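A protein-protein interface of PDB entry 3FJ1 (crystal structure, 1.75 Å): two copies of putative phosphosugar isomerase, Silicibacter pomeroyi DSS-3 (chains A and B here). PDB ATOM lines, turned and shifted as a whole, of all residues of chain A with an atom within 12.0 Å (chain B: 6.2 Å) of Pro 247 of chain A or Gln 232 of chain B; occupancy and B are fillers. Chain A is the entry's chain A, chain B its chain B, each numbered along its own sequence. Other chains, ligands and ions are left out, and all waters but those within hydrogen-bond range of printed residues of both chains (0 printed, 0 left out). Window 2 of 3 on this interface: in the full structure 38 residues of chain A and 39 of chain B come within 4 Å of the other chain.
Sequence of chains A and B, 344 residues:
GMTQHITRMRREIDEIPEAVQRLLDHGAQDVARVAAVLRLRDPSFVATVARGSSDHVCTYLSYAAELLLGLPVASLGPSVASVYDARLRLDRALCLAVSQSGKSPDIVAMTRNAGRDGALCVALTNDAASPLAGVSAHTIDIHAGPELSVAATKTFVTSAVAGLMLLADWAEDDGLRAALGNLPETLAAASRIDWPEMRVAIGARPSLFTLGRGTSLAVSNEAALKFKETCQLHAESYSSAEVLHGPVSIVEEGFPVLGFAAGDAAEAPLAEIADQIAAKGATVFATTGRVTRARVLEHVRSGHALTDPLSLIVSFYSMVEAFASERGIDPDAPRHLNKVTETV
O of Pro 247 of chain A is in hydrogen-bond range of NE2 of Gln 232 of chain B (2.8 Å).
NE2 of Gln 232 of chain B lies close to O of Lys 228 of chain B, 3.3 Å away.
O of Glu 229 of chain B sits at hydrogen-bond distance from NE2 of Gln 232 of chain B (3.3 Å).
NE2 of His 234 of chain A is in hydrogen-bond range of OE2 of Glu 236 of chain A, at 2.6 Å.
Among the printed residues, pairs that only touch across the chains: Pro 247 of chain A with Glu 229 of chain B (3.3 Å), His 234 of chain A with His 234 of chain B (3.7 Å), Pro 247 of chain A with Lys 228 of chain B (3.7 Å) and Pro 247 of chain A with Leu 225 of chain B (3.8 Å).
Of the printed residues of chain B, His 234 of chain A touches His 234 (3.7 Å).
Ala 241 of chain A touches none of the printed residues of chain B.
Of the printed residues of chain B, Pro 247 of chain A touches Leu 225, Lys 228, Glu 229 and Gln 232.
Ser 249 of chain A touches none of the printed residues of chain B.
Of the printed residues of chain A, Leu 225 of chain B touches Pro 247.
Phe 227 of chain B touches none of the printed residues of chain A.
Of the printed residues of chain A, Glu 229 of chain B touches Pro 247 (3.3 Å).
No residue of chain A comes within 4 Å of Thr 230 of chain B.
No residue of chain A comes within 4 Å of Cys 231 of chain B.
Gln 232 of chain B touches one residue of chain A.
Printed residues of chain A within 4 Å of His 234 of chain B: His 234 (3.7 Å).
The nearest printed residue of chain B that does not touch Pro 247 of chain A is Thr 230 of chain B (6.3 Å).
The nearest residue of chain A that does not touch Gln 232 of chain B is Val 248 of chain A (4.2 Å).
Hydrophobic or aromatic side chains of chain A within 4 Å of the printed part of chain B: His 234 and Pro 247.
His 234 of chain B touches its own counterpart, His 234 of chain A.
1 position is printed for both chains.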
ATOM      1  N   PHE A 209     -16.233 -23.919  28.496  1.00  0.00           N
ATOM      2  CA  PHE A 209     -17.106 -24.975  28.038  1.00  0.00           C
ATOM      3  C   PHE A 209     -16.282 -26.237  27.780  1.00  0.00           C
ATOM      4  O   PHE A 209     -15.230 -26.185  27.157  1.00  0.00           O
ATOM      5  CB  PHE A 209     -17.879 -24.579  26.778  1.00  0.00           C
ATOM      6  CG  PHE A 209     -18.779 -23.397  26.976  1.00  0.00           C
ATOM      7  CD1 PHE A 209     -19.885 -23.504  27.789  1.00  0.00           C
ATOM      8  CD2 PHE A 209     -18.531 -22.199  26.326  1.00  0.00           C
ATOM      9  CE1 PHE A 209     -20.746 -22.424  27.970  1.00  0.00           C
ATOM     10  CE2 PHE A 209     -19.365 -21.108  26.502  1.00  0.00           C
ATOM     11  CZ  PHE A 209     -20.482 -21.226  27.335  1.00  0.00           C
ATOM     12  N   LEU A 211     -16.442 -30.335  26.424  1.00  0.00           N
ATOM     13  CA  LEU A 211     -17.191 -31.259  25.603  1.00  0.00           C
ATOM     14  C   LEU A 211     -16.649 -32.670  25.749  1.00  0.00           C
ATOM     15  O   LEU A 211     -15.463 -32.897  26.001  1.00  0.00           O
ATOM     16  CB  LEU A 211     -17.124 -30.877  24.115  1.00  0.00           C
ATOM     17  CG  LEU A 211     -17.491 -29.459  23.685  1.00  0.00           C
ATOM     18  CD1 LEU A 211     -17.360 -29.342  22.117  1.00  0.00           C
ATOM     19  CD2 LEU A 211     -18.868 -29.081  24.140  1.00  0.00           C
ATOM     20  N   HIS A 234     -17.161 -19.972  36.178  1.00  0.00           N
ATOM     21  CA  HIS A 234     -18.207 -20.792  35.623  1.00  0.00           C
ATOM     22  C   HIS A 234     -17.678 -21.734  34.551  1.00  0.00           C
ATOM     23  O   HIS A 234     -16.801 -21.357  33.773  1.00  0.00           O
ATOM     24  CB  HIS A 234     -19.300 -19.901  35.022  1.00  0.00           C
ATOM     25  CG  HIS A 234     -20.485 -20.669  34.527  1.00  0.00           C
ATOM     26  ND1 HIS A 234     -21.224 -21.498  35.348  1.00  0.00           N
ATOM     27  CD2 HIS A 234     -21.058 -20.732  33.301  1.00  0.00           C
ATOM     28  CE1 HIS A 234     -22.204 -22.038  34.644  1.00  0.00           C
ATOM     29  NE2 HIS A 234     -22.121 -21.596  33.398  1.00  0.00           N
ATOM     30  N   GLU A 236     -19.337 -25.258  32.026  1.00  0.00           N
ATOM     31  CA  GLU A 236     -20.467 -26.126  31.653  1.00  0.00           C
ATOM     32  C   GLU A 236     -19.967 -27.219  30.717  1.00  0.00           C
ATOM     33  O   GLU A 236     -19.197 -26.924  29.794  1.00  0.00           O
ATOM     34  CB  GLU A 236     -21.581 -25.347  30.947  1.00  0.00           C
ATOM     35  CG  GLU A 236     -22.317 -24.331  31.797  1.00  0.00           C
ATOM     36  CD  GLU A 236     -23.290 -23.481  30.980  1.00  0.00           C
ATOM     37  OE1 GLU A 236     -23.861 -23.973  29.977  1.00  0.00           O
ATOM     38  OE2 GLU A 236     -23.483 -22.310  31.332  1.00  0.00           O
ATOM     39  N   SER A 237     -20.406 -28.453  30.968  1.00  0.00           N
ATOM     40  CA  SER A 237     -20.073 -29.605  30.151  1.00  0.00           C
ATOM     41  C   SER A 237     -21.231 -30.014  29.219  1.00  0.00           C
ATOM     42  O   SER A 237     -22.397 -30.102  29.640  1.00  0.00           O
ATOM     43  CB  SER A 237     -19.728 -30.794  31.042  1.00  0.00           C
ATOM     44  OG  SER A 237     -19.420 -31.909  30.236  1.00  0.00           O
ATOM     45  N   TYR A 238     -20.897 -30.353  27.984  1.00  0.00           N
ATOM     46  CA  TYR A 238     -21.894 -30.756  27.025  1.00  0.00           C
ATOM     47  C   TYR A 238     -21.442 -31.927  26.215  1.00  0.00           C
ATOM     48  O   TYR A 238     -20.237 -32.088  25.977  1.00  0.00           O
ATOM     49  CB  TYR A 238     -22.121 -29.643  25.996  1.00  0.00           C
ATOM     50  CG  TYR A 238     -22.766 -28.391  26.530  1.00  0.00           C
ATOM     51  CD1 TYR A 238     -22.000 -27.329  27.019  1.00  0.00           C
ATOM     52  CD2 TYR A 238     -24.129 -28.255  26.495  1.00  0.00           C
ATOM     53  CE1 TYR A 238     -22.614 -26.165  27.497  1.00  0.00           C
ATOM     54  CE2 TYR A 238     -24.735 -27.124  26.950  1.00  0.00           C
ATOM     55  CZ  TYR A 238     -23.981 -26.097  27.469  1.00  0.00           C
ATOM     56  OH  TYR A 238     -24.676 -24.976  27.915  1.00  0.00           O
ATOM     57  N   SER A 239     -22.410 -32.734  25.761  1.00  0.00           N
ATOM     58  CA  SER A 239     -22.118 -33.665  24.700  1.00  0.00           C
ATOM     59  C   SER A 239     -21.826 -32.813  23.460  1.00  0.00           C
ATOM     60  O   SER A 239     -22.571 -31.878  23.154  1.00  0.00           O
ATOM     61  CB  SER A 239     -23.306 -34.596  24.412  1.00  0.00           C
ATOM     62  OG  SER A 239     -23.054 -35.420  23.271  1.00  0.00           O
ATOM     63  N   ALA A 241     -22.424 -33.771  20.576  1.00  0.00           N
ATOM     64  CA  ALA A 241     -23.586 -34.002  19.716  1.00  0.00           C
ATOM     65  C   ALA A 241     -24.771 -33.116  20.092  1.00  0.00           C
ATOM     66  O   ALA A 241     -25.744 -33.048  19.349  1.00  0.00           O
ATOM     67  CB  ALA A 241     -23.994 -35.462  19.786  1.00  0.00           C
ATOM     68  N   GLU A 242     -24.739 -32.497  21.267  1.00  0.00           N
ATOM     69  CA  GLU A 242     -25.820 -31.633  21.703  1.00  0.00           C
ATOM     70  C   GLU A 242     -25.465 -30.163  21.810  1.00  0.00           C
ATOM     71  O   GLU A 242     -26.363 -29.319  21.862  1.00  0.00           O
ATOM     72  CB  GLU A 242     -26.309 -32.104  23.074  1.00  0.00           C
ATOM     73  CG  GLU A 242     -26.776 -33.546  23.072  1.00  0.00           C
ATOM     74  CD  GLU A 242     -28.014 -33.792  22.207  1.00  0.00           C
ATOM     75  OE1 GLU A 242     -28.754 -32.828  21.872  1.00  0.00           O
ATOM     76  OE2 GLU A 242     -28.240 -34.964  21.848  1.00  0.00           O
ATOM     77  N   VAL A 243     -24.174 -29.853  21.839  1.00  0.00           N
ATOM     78  CA  VAL A 243     -23.724 -28.474  22.121  1.00  0.00           C
ATOM     79  C   VAL A 243     -24.259 -27.439  21.132  1.00  0.00           C
ATOM     80  O   VAL A 243     -24.544 -26.295  21.517  1.00  0.00           O
ATOM     81  CB  VAL A 243     -22.193 -28.393  22.246  1.00  0.00           C
ATOM     82  CG1 VAL A 243     -21.508 -28.665  20.899  1.00  0.00           C
ATOM     83  CG2 VAL A 243     -21.792 -27.055  22.801  1.00  0.00           C
ATOM     84  N   LEU A 244     -24.423 -27.822  19.869  1.00  0.00           N
ATOM     85  CA  LEU A 244     -24.935 -26.883  18.868  1.00  0.00           C
ATOM     86  C   LEU A 244     -26.474 -26.779  18.841  1.00  0.00           C
ATOM     87  O   LEU A 244     -27.016 -26.041  18.039  1.00  0.00           O
ATOM     88  CB  LEU A 244     -24.413 -27.275  17.483  1.00  0.00           C
ATOM     89  CG  LEU A 244     -22.897 -27.232  17.341  1.00  0.00           C
ATOM     90  CD1 LEU A 244     -22.480 -27.746  15.971  1.00  0.00           C
ATOM     91  CD2 LEU A 244     -22.354 -25.825  17.611  1.00  0.00           C
ATOM     92  N   HIS A 245     -27.167 -27.487  19.728  1.00  0.00           N
ATOM     93  CA  HIS A 245     -28.640 -27.476  19.777  1.00  0.00           C
ATOM     94  C   HIS A 245     -29.203 -27.068  21.133  1.00  0.00           C
ATOM     95  O   HIS A 245     -30.388 -27.282  21.382  1.00  0.00           O
ATOM     96  CB  HIS A 245     -29.150 -28.889  19.469  1.00  0.00           C
ATOM     97  CG  HIS A 245     -28.507 -29.485  18.269  1.00  0.00           C
ATOM     98  ND1 HIS A 245     -28.938 -29.215  16.988  1.00  0.00           N
ATOM     99  CD2 HIS A 245     -27.415 -30.276  18.142  1.00  0.00           C
ATOM    100  CE1 HIS A 245     -28.155 -29.836  16.122  1.00  0.00           C
ATOM    101  NE2 HIS A 245     -27.224 -30.490  16.797  1.00  0.00           N
ATOM    102  N   GLY A 246     -28.374 -26.525  22.027  1.00  0.00           N
ATOM    103  CA  GLY A 246     -28.837 -26.186  23.388  1.00  0.00           C
ATOM    104  C   GLY A 246     -29.422 -24.775  23.524  1.00  0.00           C
ATOM    105  O   GLY A 246     -29.391 -24.000  22.571  1.00  0.00           O
ATOM    106  N   PRO A 247     -29.959 -24.441  24.722  1.00  0.00           N
ATOM    107  CA  PRO A 247     -30.569 -23.137  25.064  1.00  0.00           C
ATOM    108  C   PRO A 247     -29.759 -21.890  24.720  1.00  0.00           C
ATOM    109  O   PRO A 247     -30.335 -20.864  24.304  1.00  0.00           O
ATOM    110  CB  PRO A 247     -30.705 -23.215  26.604  1.00  0.00           C
ATOM    111  CG  PRO A 247     -29.880 -24.392  27.026  1.00  0.00           C
ATOM    112  CD  PRO A 247     -29.986 -25.342  25.890  1.00  0.00           C
ATOM    113  N   VAL A 248     -28.452 -21.961  24.934  1.00  0.00           N
ATOM    114  CA  VAL A 248     -27.575 -20.829  24.668  1.00  0.00           C
ATOM    115  C   VAL A 248     -26.569 -21.132  23.555  1.00  0.00           C
ATOM    116  O   VAL A 248     -26.137 -22.276  23.372  1.00  0.00           O
ATOM    117  CB  VAL A 248     -26.825 -20.390  25.947  1.00  0.00           C
ATOM    118  N   SER A 249     -26.220 -20.096  22.797  1.00  0.00           N
ATOM    119  CA  SER A 249     -25.247 -20.228  21.723  1.00  0.00           C
ATOM    120  C   SER A 249     -23.867 -20.250  22.323  1.00  0.00           C
ATOM    121  O   SER A 249     -23.405 -19.235  22.876  1.00  0.00           O
ATOM    122  CB  SER A 249     -25.360 -19.071  20.711  1.00  0.00           C
ATOM    123  OG  SER A 249     -24.238 -19.034  19.824  1.00  0.00           O
ATOM    124  N   ILE A 250     -23.220 -21.415  22.216  1.00  0.00           N
ATOM    125  CA  ILE A 250     -21.850 -21.607  22.669  1.00  0.00           C
ATOM    126  C   ILE A 250     -20.911 -20.602  22.013  1.00  0.00           C
ATOM    127  O   ILE A 250     -20.113 -19.992  22.694  1.00  0.00           O
ATOM    128  CB  ILE A 250     -21.356 -23.063  22.396  1.00  0.00           C
ATOM    129  CG1 ILE A 250     -20.064 -23.351  23.151  1.00  0.00           C
ATOM    130  CG2 ILE A 250     -21.189 -23.350  20.887  1.00  0.00           C
ATOM    131  CD1 ILE A 250     -19.597 -24.777  22.991  1.00  0.00           C
ATOM    132  N   VAL A 251     -21.042 -20.408  20.701  1.00  0.00           N
ATOM    133  CA  VAL A 251     -20.199 -19.458  19.964  1.00  0.00           C
ATOM    134  C   VAL A 251     -20.394 -17.991  20.400  1.00  0.00           C
ATOM    135  O   VAL A 251     -19.421 -17.245  20.589  1.00  0.00           O
ATOM    136  CB  VAL A 251     -20.475 -19.535  18.451  1.00  0.00           C
ATOM    137  CG1 VAL A 251     -19.692 -18.460  17.724  1.00  0.00           C
ATOM    138  CG2 VAL A 251     -20.159 -20.936  17.902  1.00  0.00           C
ATOM    139  N   GLU A 252     -21.648 -17.575  20.547  1.00  0.00           N
ATOM    140  CA  GLU A 252     -21.981 -16.198  20.956  1.00  0.00           C
ATOM    141  C   GLU A 252     -21.471 -15.853  22.379  1.00  0.00           C
ATOM    142  O   GLU A 252     -21.246 -14.687  22.711  1.00  0.00           O
ATOM    143  CB  GLU A 252     -23.511 -16.014  20.846  1.00  0.00           C
ATOM    144  CG  GLU A 252     -24.050 -14.589  21.041  1.00  0.00           C
ATOM    145  CD  GLU A 252     -25.578 -14.480  20.894  1.00  0.00           C
ATOM    146  OE1 GLU A 252     -26.187 -15.282  20.148  1.00  0.00           O
ATOM    147  OE2 GLU A 252     -26.175 -13.572  21.519  1.00  0.00           O
ATOM    148  N   GLU A 253     -21.286 -16.874  23.220  1.00  0.00           N
ATOM    149  CA  GLU A 253     -20.793 -16.665  24.573  1.00  0.00           C
ATOM    150  C   GLU A 253     -19.359 -16.144  24.590  1.00  0.00           C
ATOM    151  O   GLU A 253     -18.973 -15.424  25.504  1.00  0.00           O
ATOM    152  CB  GLU A 253     -20.894 -17.956  25.381  1.00  0.00           C
ATOM    153  CG  GLU A 253     -22.280 -18.252  25.885  1.00  0.00           C
ATOM    154  CD  GLU A 253     -22.649 -17.335  27.031  1.00  0.00           C
ATOM    155  OE1 GLU A 253     -22.114 -17.518  28.149  1.00  0.00           O
ATOM    156  OE2 GLU A 253     -23.458 -16.417  26.804  1.00  0.00           O
ATOM    157  N   GLY A 254     -18.577 -16.529  23.589  1.00  0.00           N
ATOM    158  CA  GLY A 254     -17.195 -16.084  23.474  1.00  0.00           C
ATOM    159  C   GLY A 254     -16.218 -16.654  24.499  1.00  0.00           C
ATOM    160  O   GLY A 254     -15.217 -16.005  24.816  1.00  0.00           O
ATOM    161  N   PHE A 255     -16.499 -17.846  25.030  1.00  0.00           N
ATOM    162  CA  PHE A 255     -15.591 -18.487  25.963  1.00  0.00           C
ATOM    163  C   PHE A 255     -14.871 -19.688  25.326  1.00  0.00           C
ATOM    164  O   PHE A 255     -15.385 -20.282  24.357  1.00  0.00           O
ATOM    165  CB  PHE A 255     -16.323 -18.911  27.227  1.00  0.00           C
ATOM    166  CG  PHE A 255     -16.925 -17.751  27.969  1.00  0.00           C
ATOM    167  CD1 PHE A 255     -16.102 -16.783  28.542  1.00  0.00           C
ATOM    168  CD2 PHE A 255     -18.298 -17.613  28.083  1.00  0.00           C
ATOM    169  CE1 PHE A 255     -16.649 -15.705  29.219  1.00  0.00           C
ATOM    170  CE2 PHE A 255     -18.854 -16.540  28.766  1.00  0.00           C
ATOM    171  CZ  PHE A 255     -18.029 -15.573  29.320  1.00  0.00           C
ATOM    172  N   LEU B 225     -33.999 -25.371  32.252  1.00  0.00           N
ATOM    173  CA  LEU B 225     -33.805 -25.436  30.804  1.00  0.00           C
ATOM    174  C   LEU B 225     -34.640 -24.391  30.057  1.00  0.00           C
ATOM    175  O   LEU B 225     -34.125 -23.634  29.212  1.00  0.00           O
ATOM    176  CB  LEU B 225     -34.136 -26.833  30.258  1.00  0.00           C
ATOM    177  CG  LEU B 225     -34.180 -27.027  28.727  1.00  0.00           C
ATOM    178  CD1 LEU B 225     -32.829 -26.610  28.120  1.00  0.00           C
ATOM    179  CD2 LEU B 225     -34.627 -28.445  28.285  1.00  0.00           C
ATOM    180  N   PHE B 227     -36.249 -21.714  31.190  1.00  0.00           N
ATOM    181  CA  PHE B 227     -35.897 -20.325  31.536  1.00  0.00           C
ATOM    182  C   PHE B 227     -34.744 -19.853  30.634  1.00  0.00           C
ATOM    183  O   PHE B 227     -34.767 -18.750  30.076  1.00  0.00           O
ATOM    184  CB  PHE B 227     -35.462 -20.251  32.985  1.00  0.00           C
ATOM    185  CG  PHE B 227     -35.178 -18.849  33.482  1.00  0.00           C
ATOM    186  CD1 PHE B 227     -36.223 -17.984  33.790  1.00  0.00           C
ATOM    187  CD2 PHE B 227     -33.884 -18.409  33.658  1.00  0.00           C
ATOM    188  CE1 PHE B 227     -35.952 -16.688  34.235  1.00  0.00           C
ATOM    189  CE2 PHE B 227     -33.612 -17.132  34.138  1.00  0.00           C
ATOM    190  CZ  PHE B 227     -34.643 -16.273  34.411  1.00  0.00           C
ATOM    191  N   LYS B 228     -33.713 -20.684  30.521  1.00  0.00           N
ATOM    192  CA  LYS B 228     -32.572 -20.387  29.645  1.00  0.00           C
ATOM    193  C   LYS B 228     -32.979 -20.220  28.185  1.00  0.00           C
ATOM    194  O   LYS B 228     -32.629 -19.222  27.548  1.00  0.00           O
ATOM    195  CB  LYS B 228     -31.496 -21.481  29.760  1.00  0.00           C
ATOM    196  CG  LYS B 228     -30.724 -21.472  31.067  1.00  0.00           C
ATOM    197  CD  LYS B 228     -29.607 -22.546  31.102  1.00  0.00           C
ATOM    198  CE  LYS B 228     -30.145 -23.938  31.048  1.00  0.00           C
ATOM    199  NZ  LYS B 228     -29.038 -24.928  31.375  1.00  0.00           N
ATOM    200  N   GLU B 229     -33.758 -21.167  27.677  1.00  0.00           N
ATOM    201  CA  GLU B 229     -34.191 -21.145  26.286  1.00  0.00           C
ATOM    202  C   GLU B 229     -35.054 -19.926  25.954  1.00  0.00           C
ATOM    203  O   GLU B 229     -34.838 -19.276  24.921  1.00  0.00           O
ATOM    204  CB  GLU B 229     -34.889 -22.473  25.908  1.00  0.00           C
ATOM    205  CG  GLU B 229     -33.901 -23.635  25.964  1.00  0.00           C
ATOM    206  CD  GLU B 229     -34.304 -24.937  25.303  1.00  0.00           C
ATOM    207  OE1 GLU B 229     -35.453 -25.386  25.429  1.00  0.00           O
ATOM    208  OE2 GLU B 229     -33.398 -25.544  24.700  1.00  0.00           O
ATOM    209  N   THR B 230     -35.999 -19.599  26.825  1.00  0.00           N
ATOM    210  CA  THR B 230     -36.923 -18.526  26.523  1.00  0.00           C
ATOM    211  C   THR B 230     -36.383 -17.125  26.813  1.00  0.00           C
ATOM    212  O   THR B 230     -36.633 -16.199  26.048  1.00  0.00           O
ATOM    213  CB  THR B 230     -38.274 -18.724  27.248  1.00  0.00           C
ATOM    214  OG1 THR B 230     -38.049 -18.766  28.642  1.00  0.00           O
ATOM    215  CG2 THR B 230     -38.955 -20.004  26.824  1.00  0.00           C
ATOM    216  N   CYS B 231     -35.649 -16.986  27.909  1.00  0.00           N
ATOM    217  CA  CYS B 231     -35.151 -15.676  28.340  1.00  0.00           C
ATOM    218  C   CYS B 231     -33.685 -15.383  28.042  1.00  0.00           C
ATOM    219  O   CYS B 231     -33.261 -14.234  28.184  1.00  0.00           O
ATOM    220  CB  CYS B 231     -35.379 -15.513  29.840  1.00  0.00           C
ATOM    221  SG  CYS B 231     -37.112 -15.593  30.331  1.00  0.00           S
ATOM    222  N   GLN B 232     -32.895 -16.394  27.685  1.00  0.00           N
ATOM    223  CA  GLN B 232     -31.489 -16.179  27.427  1.00  0.00           C
ATOM    224  C   GLN B 232     -30.763 -15.611  28.672  1.00  0.00           C
ATOM    225  O   GLN B 232     -29.881 -14.766  28.555  1.00  0.00           O
ATOM    226  CB  GLN B 232     -31.291 -15.287  26.185  1.00  0.00           C
ATOM    227  CG  GLN B 232     -31.766 -15.958  24.879  1.00  0.00           C
ATOM    228  CD  GLN B 232     -30.988 -17.227  24.580  1.00  0.00           C
ATOM    229  OE1 GLN B 232     -29.751 -17.194  24.411  1.00  0.00           O
ATOM    230  NE2 GLN B 232     -31.696 -18.381  24.543  1.00  0.00           N
ATOM    231  N   LEU B 233     -31.166 -16.109  29.848  1.00  0.00           N
ATOM    232  CA  LEU B 233     -30.617 -15.759  31.150  1.00  0.00           C
ATOM    233  C   LEU B 233     -30.234 -17.094  31.806  1.00  0.00           C
ATOM    234  O   LEU B 233     -30.828 -18.127  31.481  1.00  0.00           O
ATOM    235  CB  LEU B 233     -31.674 -15.025  32.003  1.00  0.00           C
ATOM    236  CG  LEU B 233     -32.061 -13.626  31.492  1.00  0.00           C
ATOM    237  CD1 LEU B 233     -33.297 -13.117  32.209  1.00  0.00           C
ATOM    238  CD2 LEU B 233     -30.857 -12.648  31.597  1.00  0.00           C
ATOM    239  N   HIS B 234     -29.238 -17.069  32.679  1.00  0.00           N
ATOM    240  CA  HIS B 234     -28.727 -18.272  33.290  1.00  0.00           C
ATOM    241  C   HIS B 234     -29.657 -18.861  34.319  1.00  0.00           C
ATOM    242  O   HIS B 234     -30.293 -18.136  35.090  1.00  0.00           O
ATOM    243  CB  HIS B 234     -27.386 -18.002  33.982  1.00  0.00           C
ATOM    244  CG  HIS B 234     -26.721 -19.239  34.515  1.00  0.00           C
ATOM    245  ND1 HIS B 234     -26.390 -20.317  33.714  1.00  0.00           N
ATOM    246  CD2 HIS B 234     -26.304 -19.556  35.764  1.00  0.00           C
ATOM    247  CE1 HIS B 234     -25.791 -21.236  34.452  1.00  0.00           C
ATOM    248  NE2 HIS B 234     -25.725 -20.798  35.696  1.00  0.00           N
ATOM    249  N   ILE B 329     -38.712  -9.203  26.218  1.00  0.00           N
ATOM    250  CA  ILE B 329     -38.068 -10.383  25.660  1.00  0.00           C
ATOM    251  C   ILE B 329     -39.125 -11.166  24.877  1.00  0.00           C
ATOM    252  O   ILE B 329     -40.183 -11.513  25.409  1.00  0.00           O
ATOM    253  CB  ILE B 329     -37.474 -11.322  26.733  1.00  0.00           C
ATOM    254  CG1 ILE B 329     -36.479 -10.579  27.636  1.00  0.00           C
ATOM    255  CG2 ILE B 329     -36.790 -12.512  26.062  1.00  0.00           C
ATOM    256  CD1 ILE B 329     -36.063 -11.380  28.848  1.00  0.00           C
